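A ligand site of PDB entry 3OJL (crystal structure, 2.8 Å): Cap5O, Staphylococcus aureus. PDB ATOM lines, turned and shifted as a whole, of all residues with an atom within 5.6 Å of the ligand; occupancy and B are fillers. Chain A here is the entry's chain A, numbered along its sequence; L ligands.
O2 of the ligand is in hydrogen-bond range of N of Tyr 21 (3.1 Å).
O9 of the ligand sits at hydrogen-bond distance from N of Ile 22 (3.1 Å).
N of Ile 42 sits at hydrogen-bond distance from N5 of the ligand.
The side-chain hydroxyl (OG1) of Thr 93 lies within hydrogen-bond range of an oxygen (O13) of the ligand (2.6 Å).
The backbone NH (N) of Gly 20 lies close to an oxygen (O3) of the ligand, at 3.5 Å.
O12 of the ligand sits at hydrogen-bond distance from N of Thr 93.
An oxygen (O13) of the ligand is in hydrogen-bond range of the side-chain hydroxyl (OG1) of Thr 130 (3.0 Å).
The backbone NH of Thr 130 sits at hydrogen-bond distance from an oxygen (O13) of the ligand (2.8 Å).
An oxygen (O5) of the ligand sits at hydrogen-bond distance from the side-chain carboxylate (OD2) of Asp 41, at 2.5 Å.
O of Thr 130 is in hydrogen-bond range of OG1 of Thr 93 (3.0 Å).
N of Gly 18 lies within hydrogen-bond range of O of Val 40, 2.8 Å away.
O of Glu 128 lies within hydrogen-bond range of N of Glu 162, 3.3 Å away.
The backbone carbonyl oxygen (O) of Val 17 lies within hydrogen-bond range of the backbone NH (N) of Ala 90 (2.8 Å).
The side-chain carboxylate of Asp 41 lies within hydrogen-bond range of the backbone NH of Asn 43.
OG of Ser 129 lies within hydrogen-bond range of O of Val 91 (2.7 Å).
OG of Ser 114 sits at hydrogen-bond distance from O of Ala 111.
OD2 of Asp 41 sits at hydrogen-bond distance from N of Leu 19, 2.9 Å away.
Residues that only touch the ligand: Val 17 (3.3 Å), Gly 18 (3.1 Å), Leu 19 (3.7 Å), Asn 43 (3.95 Å), Ala 90 (3.97 Å), Val 91 (3.4 Å), Pro 92 (3.1 Å), Leu 107 (3.6 Å), Arg 110 (3.6 Å), Ala 111 (3.7 Å), Ser 129 (3.8 Å), Glu 162 (3.7 Å), Arg 163 (3.8 Å), Val 164 (3.6 Å) and Cys 269 (3.5 Å).
Hydrophobic or aromatic side chains that line the ligand: Val 17, Tyr 21, Ile 22, Ile 42, Val 91, Pro 92, Leu 107 and Val 164.
Within 4 Å of the ligand: Val 17, Gly 18, Leu 19, Gly 20, Tyr 21, Ile 22, Asp 41, Ile 42, Asn 43, Ala 90, Val 91, Pro 92, Thr 93, Leu 107, Arg 110, Ala 111, Ser 129, Thr 130, Glu 162, Arg 163, Val 164 and Cys 269.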
ATOM      1  N   VAL A  17     -19.335 -12.663  28.218  1.00  0.00           N
ATOM      2  CA  VAL A  17     -18.733 -11.346  28.053  1.00  0.00           C
ATOM      3  C   VAL A  17     -19.872 -10.343  27.984  1.00  0.00           C
ATOM      4  O   VAL A  17     -20.732 -10.447  27.125  1.00  0.00           O
ATOM      5  CB  VAL A  17     -17.792 -11.301  26.816  1.00  0.00           C
ATOM      6  CG1 VAL A  17     -17.135  -9.938  26.694  1.00  0.00           C
ATOM      7  CG2 VAL A  17     -16.722 -12.405  26.900  1.00  0.00           C
ATOM      8  N   GLY A  18     -19.884  -9.367  28.897  1.00  0.00           N
ATOM      9  CA  GLY A  18     -21.001  -8.425  28.996  1.00  0.00           C
ATOM     10  C   GLY A  18     -21.984  -8.978  30.010  1.00  0.00           C
ATOM     11  O   GLY A  18     -22.624  -9.993  29.763  1.00  0.00           O
ATOM     12  N   LEU A  19     -22.009  -8.393  31.216  1.00  0.00           N
ATOM     13  CA  LEU A  19     -22.830  -8.850  32.331  1.00  0.00           C
ATOM     14  C   LEU A  19     -23.910  -7.847  32.730  1.00  0.00           C
ATOM     15  O   LEU A  19     -24.039  -7.518  33.913  1.00  0.00           O
ATOM     16  CB  LEU A  19     -21.936  -9.190  33.523  1.00  0.00           C
ATOM     17  CG  LEU A  19     -20.953 -10.339  33.371  1.00  0.00           C
ATOM     18  CD1 LEU A  19     -19.965 -10.301  34.494  1.00  0.00           C
ATOM     19  CD2 LEU A  19     -21.654 -11.686  33.324  1.00  0.00           C
ATOM     20  N   GLY A  20     -24.692  -7.394  31.739  1.00  0.00           N
ATOM     21  CA  GLY A  20     -25.824  -6.488  31.924  1.00  0.00           C
ATOM     22  C   GLY A  20     -27.133  -7.237  32.102  1.00  0.00           C
ATOM     23  O   GLY A  20     -27.124  -8.361  32.610  1.00  0.00           O
ATOM     24  N   TYR A  21     -28.260  -6.628  31.656  1.00  0.00           N
ATOM     25  CA  TYR A  21     -29.594  -7.244  31.716  1.00  0.00           C
ATOM     26  C   TYR A  21     -29.676  -8.632  31.026  1.00  0.00           C
ATOM     27  O   TYR A  21     -30.584  -9.406  31.347  1.00  0.00           O
ATOM     28  CB  TYR A  21     -30.678  -6.293  31.155  1.00  0.00           C
ATOM     29  CG  TYR A  21     -31.175  -5.269  32.157  1.00  0.00           C
ATOM     30  CD1 TYR A  21     -31.864  -5.662  33.296  1.00  0.00           C
ATOM     31  CD2 TYR A  21     -30.971  -3.914  31.943  1.00  0.00           C
ATOM     32  CE1 TYR A  21     -32.336  -4.717  34.214  1.00  0.00           C
ATOM     33  CE2 TYR A  21     -31.444  -2.962  32.845  1.00  0.00           C
ATOM     34  CZ  TYR A  21     -32.116  -3.371  33.990  1.00  0.00           C
ATOM     35  OH  TYR A  21     -32.583  -2.443  34.895  1.00  0.00           O
ATOM     36  N   ILE A  22     -28.737  -8.951  30.113  1.00  0.00           N
ATOM     37  CA  ILE A  22     -28.656 -10.229  29.417  1.00  0.00           C
ATOM     38  C   ILE A  22     -27.595 -11.126  30.050  1.00  0.00           C
ATOM     39  O   ILE A  22     -27.917 -12.238  30.473  1.00  0.00           O
ATOM     40  CB  ILE A  22     -28.417 -10.042  27.891  1.00  0.00           C
ATOM     41  CG1 ILE A  22     -29.523  -9.238  27.220  1.00  0.00           C
ATOM     42  CG2 ILE A  22     -28.162 -11.378  27.169  1.00  0.00           C
ATOM     43  CD1 ILE A  22     -30.918  -9.856  27.260  1.00  0.00           C
ATOM     44  N   GLY A  23     -26.352 -10.666  30.059  1.00  0.00           N
ATOM     45  CA  GLY A  23     -25.207 -11.418  30.539  1.00  0.00           C
ATOM     46  C   GLY A  23     -25.312 -11.942  31.948  1.00  0.00           C
ATOM     47  O   GLY A  23     -25.077 -13.139  32.178  1.00  0.00           O
ATOM     48  N   VAL A  40     -17.450 -11.945  32.667  1.00  0.00           N
ATOM     49  CA  VAL A  40     -16.444 -10.952  32.236  1.00  0.00           C
ATOM     50  C   VAL A  40     -17.120  -9.640  31.846  1.00  0.00           C
ATOM     51  O   VAL A  40     -18.075  -9.659  31.068  1.00  0.00           O
ATOM     52  CB  VAL A  40     -15.527 -11.492  31.113  1.00  0.00           C
ATOM     53  CG1 VAL A  40     -14.478 -10.466  30.702  1.00  0.00           C
ATOM     54  CG2 VAL A  40     -14.858 -12.815  31.529  1.00  0.00           C
ATOM     55  N   ASP A  41     -16.634  -8.515  32.403  1.00  0.00           N
ATOM     56  CA  ASP A  41     -17.200  -7.205  32.086  1.00  0.00           C
ATOM     57  C   ASP A  41     -16.127  -6.127  32.009  1.00  0.00           C
ATOM     58  O   ASP A  41     -15.113  -6.247  32.704  1.00  0.00           O
ATOM     59  CB  ASP A  41     -18.281  -6.830  33.105  1.00  0.00           C
ATOM     60  CG  ASP A  41     -19.270  -5.810  32.572  1.00  0.00           C
ATOM     61  OD1 ASP A  41     -18.931  -4.609  32.562  1.00  0.00           O
ATOM     62  OD2 ASP A  41     -20.391  -6.210  32.213  1.00  0.00           O
ATOM     63  N   ILE A  42     -16.326  -5.081  31.152  1.00  0.00           N
ATOM     64  CA  ILE A  42     -15.373  -3.966  31.030  1.00  0.00           C
ATOM     65  C   ILE A  42     -15.449  -3.082  32.268  1.00  0.00           C
ATOM     66  O   ILE A  42     -14.467  -2.402  32.584  1.00  0.00           O
ATOM     67  CB  ILE A  42     -15.427  -3.101  29.721  1.00  0.00           C
ATOM     68  CG1 ILE A  42     -16.838  -2.572  29.364  1.00  0.00           C
ATOM     69  CG2 ILE A  42     -14.709  -3.758  28.563  1.00  0.00           C
ATOM     70  CD1 ILE A  42     -16.907  -1.221  28.432  1.00  0.00           C
ATOM     71  N   ASN A  43     -16.601  -3.103  32.980  1.00  0.00           N
ATOM     72  CA  ASN A  43     -16.804  -2.262  34.158  1.00  0.00           C
ATOM     73  C   ASN A  43     -16.297  -2.832  35.472  1.00  0.00           C
ATOM     74  O   ASN A  43     -16.811  -3.856  35.959  1.00  0.00           O
ATOM     75  CB  ASN A  43     -18.253  -1.765  34.257  1.00  0.00           C
ATOM     76  CG  ASN A  43     -18.351  -0.328  34.700  1.00  0.00           C
ATOM     77  OD1 ASN A  43     -17.452   0.228  35.359  1.00  0.00           O
ATOM     78  ND2 ASN A  43     -19.460   0.305  34.327  1.00  0.00           N
ATOM     79  N   THR A  46     -19.105  -2.754  38.209  1.00  0.00           N
ATOM     80  CA  THR A  46     -19.922  -3.955  38.037  1.00  0.00           C
ATOM     81  C   THR A  46     -19.189  -5.187  38.591  1.00  0.00           C
ATOM     82  O   THR A  46     -19.807  -5.938  39.330  1.00  0.00           O
ATOM     83  CB  THR A  46     -20.419  -4.049  36.571  1.00  0.00           C
ATOM     84  OG1 THR A  46     -21.316  -2.955  36.312  1.00  0.00           O
ATOM     85  CG2 THR A  46     -21.133  -5.343  36.266  1.00  0.00           C
ATOM     86  N   ILE A  57     -27.914  -5.400  38.093  1.00  0.00           N
ATOM     87  CA  ILE A  57     -29.198  -4.998  37.519  1.00  0.00           C
ATOM     88  C   ILE A  57     -30.402  -5.271  38.445  1.00  0.00           C
ATOM     89  O   ILE A  57     -30.403  -6.275  39.159  1.00  0.00           O
ATOM     90  CB  ILE A  57     -29.421  -5.587  36.094  1.00  0.00           C
ATOM     91  CG1 ILE A  57     -29.150  -7.098  36.031  1.00  0.00           C
ATOM     92  CG2 ILE A  57     -28.643  -4.808  35.027  1.00  0.00           C
ATOM     93  CD1 ILE A  57     -30.372  -7.908  35.927  1.00  0.00           C
ATOM     94  N   ALA A  90     -22.574 -11.026  25.110  1.00  0.00           N
ATOM     95  CA  ALA A  90     -23.839 -10.388  25.498  1.00  0.00           C
ATOM     96  C   ALA A  90     -23.606  -8.936  25.849  1.00  0.00           C
ATOM     97  O   ALA A  90     -24.113  -8.415  26.842  1.00  0.00           O
ATOM     98  CB  ALA A  90     -24.451 -11.137  26.675  1.00  0.00           C
ATOM     99  N   VAL A  91     -22.853  -8.272  24.966  1.00  0.00           N
ATOM    100  CA  VAL A  91     -22.474  -6.867  25.096  1.00  0.00           C
ATOM    101  C   VAL A  91     -23.500  -6.002  24.324  1.00  0.00           C
ATOM    102  O   VAL A  91     -24.223  -6.548  23.492  1.00  0.00           O
ATOM    103  CB  VAL A  91     -20.979  -6.618  24.701  1.00  0.00           C
ATOM    104  CG1 VAL A  91     -20.045  -7.524  25.507  1.00  0.00           C
ATOM    105  CG2 VAL A  91     -20.744  -6.822  23.212  1.00  0.00           C
ATOM    106  N   PRO A  92     -23.617  -4.677  24.590  1.00  0.00           N
ATOM    107  CA  PRO A  92     -24.635  -3.908  23.883  1.00  0.00           C
ATOM    108  C   PRO A  92     -24.314  -3.646  22.425  1.00  0.00           C
ATOM    109  O   PRO A  92     -23.146  -3.670  22.007  1.00  0.00           O
ATOM    110  CB  PRO A  92     -24.706  -2.598  24.668  1.00  0.00           C
ATOM    111  CG  PRO A  92     -23.860  -2.772  25.861  1.00  0.00           C
ATOM    112  CD  PRO A  92     -22.868  -3.821  25.525  1.00  0.00           C
ATOM    113  N   THR A  93     -25.386  -3.425  21.648  1.00  0.00           N
ATOM    114  CA  THR A  93     -25.273  -3.085  20.237  1.00  0.00           C
ATOM    115  C   THR A  93     -26.011  -1.770  19.999  1.00  0.00           C
ATOM    116  O   THR A  93     -27.204  -1.757  19.725  1.00  0.00           O
ATOM    117  CB  THR A  93     -25.683  -4.223  19.318  1.00  0.00           C
ATOM    118  OG1 THR A  93     -27.025  -4.603  19.601  1.00  0.00           O
ATOM    119  CG2 THR A  93     -24.758  -5.400  19.411  1.00  0.00           C
ATOM    120  N   PRO A  94     -25.297  -0.650  20.170  1.00  0.00           N
ATOM    121  CA  PRO A  94     -25.950   0.656  19.945  1.00  0.00           C
ATOM    122  C   PRO A  94     -26.224   0.962  18.481  1.00  0.00           C
ATOM    123  O   PRO A  94     -25.739   0.286  17.581  1.00  0.00           O
ATOM    124  CB  PRO A  94     -24.972   1.662  20.565  1.00  0.00           C
ATOM    125  CG  PRO A  94     -23.675   0.960  20.664  1.00  0.00           C
ATOM    126  CD  PRO A  94     -23.863  -0.506  20.519  1.00  0.00           C
ATOM    127  N   LEU A 107     -18.790  -3.169  19.819  1.00  0.00           N
ATOM    128  CA  LEU A 107     -18.657  -3.786  21.130  1.00  0.00           C
ATOM    129  C   LEU A 107     -18.504  -5.293  21.064  1.00  0.00           C
ATOM    130  O   LEU A 107     -17.770  -5.854  21.885  1.00  0.00           O
ATOM    131  CB  LEU A 107     -19.760  -3.356  22.073  1.00  0.00           C
ATOM    132  CG  LEU A 107     -19.568  -1.950  22.638  1.00  0.00           C
ATOM    133  CD1 LEU A 107     -20.744  -1.542  23.478  1.00  0.00           C
ATOM    134  CD2 LEU A 107     -18.265  -1.859  23.467  1.00  0.00           C
ATOM    135  N   ARG A 110     -14.658  -5.895  19.867  1.00  0.00           N
ATOM    136  CA  ARG A 110     -13.677  -5.862  20.964  1.00  0.00           C
ATOM    137  C   ARG A 110     -13.885  -7.036  21.953  1.00  0.00           C
ATOM    138  O   ARG A 110     -12.888  -7.575  22.418  1.00  0.00           O
ATOM    139  CB  ARG A 110     -13.517  -4.475  21.608  1.00  0.00           C
ATOM    140  CG  ARG A 110     -14.799  -3.827  22.118  1.00  0.00           C
ATOM    141  CD  ARG A 110     -14.633  -2.327  22.309  1.00  0.00           C
ATOM    142  NE  ARG A 110     -14.032  -1.976  23.612  1.00  0.00           N
ATOM    143  CZ  ARG A 110     -14.064  -0.756  24.139  1.00  0.00           C
ATOM    144  NH1 ARG A 110     -14.672   0.242  23.499  1.00  0.00           N
ATOM    145  NH2 ARG A 110     -13.489  -0.520  25.312  1.00  0.00           N
ATOM    146  N   ALA A 111     -15.164  -7.466  22.234  1.00  0.00           N
ATOM    147  CA  ALA A 111     -15.447  -8.683  23.044  1.00  0.00           C
ATOM    148  C   ALA A 111     -14.866  -9.900  22.349  1.00  0.00           C
ATOM    149  O   ALA A 111     -14.272 -10.759  22.985  1.00  0.00           O
ATOM    150  CB  ALA A 111     -16.943  -8.879  23.236  1.00  0.00           C
ATOM    151  N   SER A 114     -11.062  -9.950  22.802  1.00  0.00           N
ATOM    152  CA  SER A 114     -10.741 -10.376  24.153  1.00  0.00           C
ATOM    153  C   SER A 114     -10.846 -11.929  24.371  1.00  0.00           C
ATOM    154  O   SER A 114     -10.170 -12.478  25.266  1.00  0.00           O
ATOM    155  CB  SER A 114     -11.603  -9.615  25.155  1.00  0.00           C
ATOM    156  OG  SER A 114     -12.968  -9.967  25.038  1.00  0.00           O
ATOM    157  N   GLU A 128     -25.051 -13.365  21.414  1.00  0.00           N
ATOM    158  CA  GLU A 128     -26.401 -13.140  21.955  1.00  0.00           C
ATOM    159  C   GLU A 128     -26.877 -11.730  21.685  1.00  0.00           C
ATOM    160  O   GLU A 128     -28.075 -11.453  21.770  1.00  0.00           O
ATOM    161  CB  GLU A 128     -26.451 -13.423  23.458  1.00  0.00           C
ATOM    162  CG  GLU A 128     -26.584 -14.906  23.799  1.00  0.00           C
ATOM    163  CD  GLU A 128     -26.956 -15.206  25.248  1.00  0.00           C
ATOM    164  OE1 GLU A 128     -26.668 -14.354  26.125  1.00  0.00           O
ATOM    165  OE2 GLU A 128     -27.499 -16.299  25.493  1.00  0.00           O
ATOM    166  N   SER A 129     -25.942 -10.839  21.382  1.00  0.00           N
ATOM    167  CA  SER A 129     -26.189  -9.441  21.054  1.00  0.00           C
ATOM    168  C   SER A 129     -26.936  -9.349  19.719  1.00  0.00           C
ATOM    169  O   SER A 129     -26.802 -10.233  18.874  1.00  0.00           O
ATOM    170  CB  SER A 129     -24.876  -8.697  20.941  1.00  0.00           C
ATOM    171  OG  SER A 129     -24.046  -8.894  22.076  1.00  0.00           O
ATOM    172  N   THR A 130     -27.714  -8.272  19.532  1.00  0.00           N
ATOM    173  CA  THR A 130     -28.451  -8.053  18.300  1.00  0.00           C
ATOM    174  C   THR A 130     -27.455  -7.600  17.232  1.00  0.00           C
ATOM    175  O   THR A 130     -26.709  -6.649  17.444  1.00  0.00           O
ATOM    176  CB  THR A 130     -29.602  -7.098  18.548  1.00  0.00           C
ATOM    177  OG1 THR A 130     -30.321  -7.555  19.693  1.00  0.00           O
ATOM    178  CG2 THR A 130     -30.546  -7.029  17.394  1.00  0.00           C
ATOM    179  N   GLU A 162     -30.801 -13.277  22.125  1.00  0.00           N
ATOM    180  CA  GLU A 162     -31.461 -13.331  23.430  1.00  0.00           C
ATOM    181  C   GLU A 162     -32.174 -12.016  23.692  1.00  0.00           C
ATOM    182  O   GLU A 162     -31.562 -10.942  23.594  1.00  0.00           O
ATOM    183  CB  GLU A 162     -30.464 -13.664  24.562  1.00  0.00           C
ATOM    184  CG  GLU A 162     -31.072 -14.431  25.726  1.00  0.00           C
ATOM    185  CD  GLU A 162     -30.661 -15.899  25.854  1.00  0.00           C
ATOM    186  OE1 GLU A 162     -30.075 -16.267  26.894  1.00  0.00           O
ATOM    187  OE2 GLU A 162     -30.939 -16.684  24.911  1.00  0.00           O
ATOM    188  N   ARG A 163     -33.467 -12.118  23.996  1.00  0.00           N
ATOM    189  CA  ARG A 163     -34.347 -11.004  24.296  1.00  0.00           C
ATOM    190  C   ARG A 163     -35.115 -11.376  25.582  1.00  0.00           C
ATOM    191  O   ARG A 163     -35.548 -12.526  25.715  1.00  0.00           O
ATOM    192  CB  ARG A 163     -35.313 -10.793  23.094  1.00  0.00           C
ATOM    193  CG  ARG A 163     -36.209  -9.559  23.162  1.00  0.00           C
ATOM    194  CD  ARG A 163     -37.546  -9.812  22.460  1.00  0.00           C
ATOM    195  NE  ARG A 163     -37.473  -9.682  20.999  1.00  0.00           N
ATOM    196  CZ  ARG A 163     -38.468  -9.993  20.162  1.00  0.00           C
ATOM    197  NH1 ARG A 163     -39.601 -10.485  20.628  1.00  0.00           N
ATOM    198  NH2 ARG A 163     -38.311  -9.822  18.850  1.00  0.00           N
ATOM    199  N   VAL A 164     -35.236 -10.451  26.550  1.00  0.00           N
ATOM    200  CA  VAL A 164     -35.951 -10.719  27.811  1.00  0.00           C
ATOM    201  C   VAL A 164     -36.751  -9.517  28.334  1.00  0.00           C
ATOM    202  O   VAL A 164     -36.294  -8.380  28.270  1.00  0.00           O
ATOM    203  CB  VAL A 164     -35.113 -11.367  28.945  1.00  0.00           C
ATOM    204  CG1 VAL A 164     -34.972 -12.880  28.763  1.00  0.00           C
ATOM    205  CG2 VAL A 164     -33.767 -10.685  29.132  1.00  0.00           C
ATOM    206  N   HIS A 268     -36.683  -0.459  23.354  1.00  0.00           N
ATOM    207  CA  HIS A 268     -35.257  -0.607  23.114  1.00  0.00           C
ATOM    208  C   HIS A 268     -35.138  -1.250  21.725  1.00  0.00           C
ATOM    209  O   HIS A 268     -34.746  -0.551  20.792  1.00  0.00           O
ATOM    210  CB  HIS A 268     -34.557  -1.438  24.229  1.00  0.00           C
ATOM    211  CG  HIS A 268     -33.382  -0.752  24.882  1.00  0.00           C
ATOM    212  ND1 HIS A 268     -33.431   0.587  25.290  1.00  0.00           N
ATOM    213  CD2 HIS A 268     -32.180  -1.269  25.247  1.00  0.00           C
ATOM    214  CE1 HIS A 268     -32.260   0.835  25.855  1.00  0.00           C
ATOM    215  NE2 HIS A 268     -31.477  -0.251  25.863  1.00  0.00           N
ATOM    216  N   CYS A 269     -35.671  -2.491  21.552  1.00  0.00           N
ATOM    217  CA  CYS A 269     -35.663  -3.239  20.296  1.00  0.00           C
ATOM    218  C   CYS A 269     -36.464  -2.596  19.160  1.00  0.00           C
ATOM    219  O   CYS A 269     -35.924  -2.453  18.068  1.00  0.00           O
ATOM    220  CB  CYS A 269     -36.070  -4.696  20.526  1.00  0.00           C
ATOM    221  SG  CYS A 269     -34.709  -5.902  20.408  1.00  0.00           S
ATOM    222  N   ARG A 333     -36.341   6.015  29.199  1.00  0.00           N
ATOM    223  CA  ARG A 333     -35.171   6.007  28.300  1.00  0.00           C
ATOM    224  C   ARG A 333     -35.407   5.845  26.784  1.00  0.00           C
ATOM    225  O   ARG A 333     -34.741   6.512  25.978  1.00  0.00           O
ATOM    226  CB  ARG A 333     -33.984   5.151  28.830  1.00  0.00           C
ATOM    227  CG  ARG A 333     -34.271   3.705  29.232  1.00  0.00           C
ATOM    228  CD  ARG A 333     -33.009   2.994  29.715  1.00  0.00           C
ATOM    229  NE  ARG A 333     -33.204   1.549  29.904  1.00  0.00           N
ATOM    230  CZ  ARG A 333     -32.232   0.635  29.850  1.00  0.00           C
ATOM    231  NH1 ARG A 333     -30.984   1.006  29.595  1.00  0.00           N
ATOM    232  NH2 ARG A 333     -32.504  -0.654  30.042  1.00  0.00           N
HETATM  233  P1  LIG L   1     -26.309  -3.720  29.405  1.00  0.00           P
HETATM  234  O1  LIG L   1     -25.872  -2.306  29.263  1.00  0.00           O
HETATM  235  O2  LIG L   1     -27.274  -3.879  30.525  1.00  0.00           O
HETATM  236  O3  LIG L   1     -25.000  -4.629  29.654  1.00  0.00           O
HETATM  237  C1  LIG L   1     -23.897  -4.691  28.784  1.00  0.00           C
HETATM  238  C2  LIG L   1     -22.708  -5.084  29.638  1.00  0.00           C
HETATM  239  O4  LIG L   1     -21.614  -5.399  28.806  1.00  0.00           O
HETATM  240  C3  LIG L   1     -22.254  -3.925  30.534  1.00  0.00           C
HETATM  241  O5  LIG L   1     -22.123  -4.403  31.860  1.00  0.00           O
HETATM  242  C4  LIG L   1     -20.907  -3.508  29.960  1.00  0.00           C
HETATM  243  O6  LIG L   1     -20.058  -2.989  30.961  1.00  0.00           O
HETATM  244  C5  LIG L   1     -20.442  -4.814  29.336  1.00  0.00           C
HETATM  245  N1  LIG L   1     -19.494  -4.644  28.226  1.00  0.00           N
HETATM  246  C6  LIG L   1     -19.622  -3.797  27.173  1.00  0.00           C
HETATM  247  N2  LIG L   1     -18.586  -4.012  26.333  1.00  0.00           N
HETATM  248  C7  LIG L   1     -17.818  -5.002  26.806  1.00  0.00           C
HETATM  249  C8  LIG L   1     -16.656  -5.614  26.325  1.00  0.00           C
HETATM  250  N3  LIG L   1     -16.144  -5.299  25.130  1.00  0.00           N
HETATM  251  N4  LIG L   1     -16.073  -6.627  27.072  1.00  0.00           N
HETATM  252  C9  LIG L   1     -16.676  -7.042  28.257  1.00  0.00           C
HETATM  253  N5  LIG L   1     -17.833  -6.427  28.714  1.00  0.00           N
HETATM  254  C10 LIG L   1     -18.392  -5.427  27.999  1.00  0.00           C
HETATM  255  O7  LIG L   1     -26.893  -4.281  28.020  1.00  0.00           O
HETATM  256  P2  LIG L   1     -27.951  -5.498  27.952  1.00  0.00           P
HETATM  257  O8  LIG L   1     -29.259  -5.000  28.450  1.00  0.00           O
HETATM  258  O9  LIG L   1     -27.341  -6.716  28.532  1.00  0.00           O
HETATM  259  O10 LIG L   1     -28.150  -5.751  26.366  1.00  0.00           O
HETATM  260  C11 LIG L   1     -27.097  -6.151  25.530  1.00  0.00           C
HETATM  261  C12 LIG L   1     -27.598  -6.355  24.107  1.00  0.00           C
HETATM  262  O11 LIG L   1     -28.452  -7.478  24.000  1.00  0.00           O
HETATM  263  C13 LIG L   1     -28.413  -5.199  23.522  1.00  0.00           C
HETATM  264  O12 LIG L   1     -27.654  -4.096  23.078  1.00  0.00           O
HETATM  265  C14 LIG L   1     -29.111  -5.903  22.374  1.00  0.00           C
HETATM  266  O13 LIG L   1     -28.173  -6.182  21.365  1.00  0.00           O
HETATM  267  C15 LIG L   1     -29.457  -7.231  23.020  1.00  0.00           C
HETATM  268  N6  LIG L   1     -30.821  -7.148  23.589  1.00  0.00           N
HETATM  269  C16 LIG L   1     -31.002  -6.864  24.929  1.00  0.00           C
HETATM  270  C17 LIG L   1     -32.292  -6.785  25.478  1.00  0.00           C
HETATM  271  C18 LIG L   1     -32.436  -6.305  26.887  1.00  0.00           C
HETATM  272  O14 LIG L   1     -32.926  -7.210  27.861  1.00  0.00           O
HETATM  273  N7  LIG L   1     -32.097  -5.045  27.195  1.00  0.00           N
HETATM  274  C19 LIG L   1     -33.401  -6.996  24.665  1.00  0.00           C
HETATM  275  C20 LIG L   1     -33.220  -7.286  23.304  1.00  0.00           C
HETATM  276  C21 LIG L   1     -31.919  -7.339  22.785  1.00  0.00           C
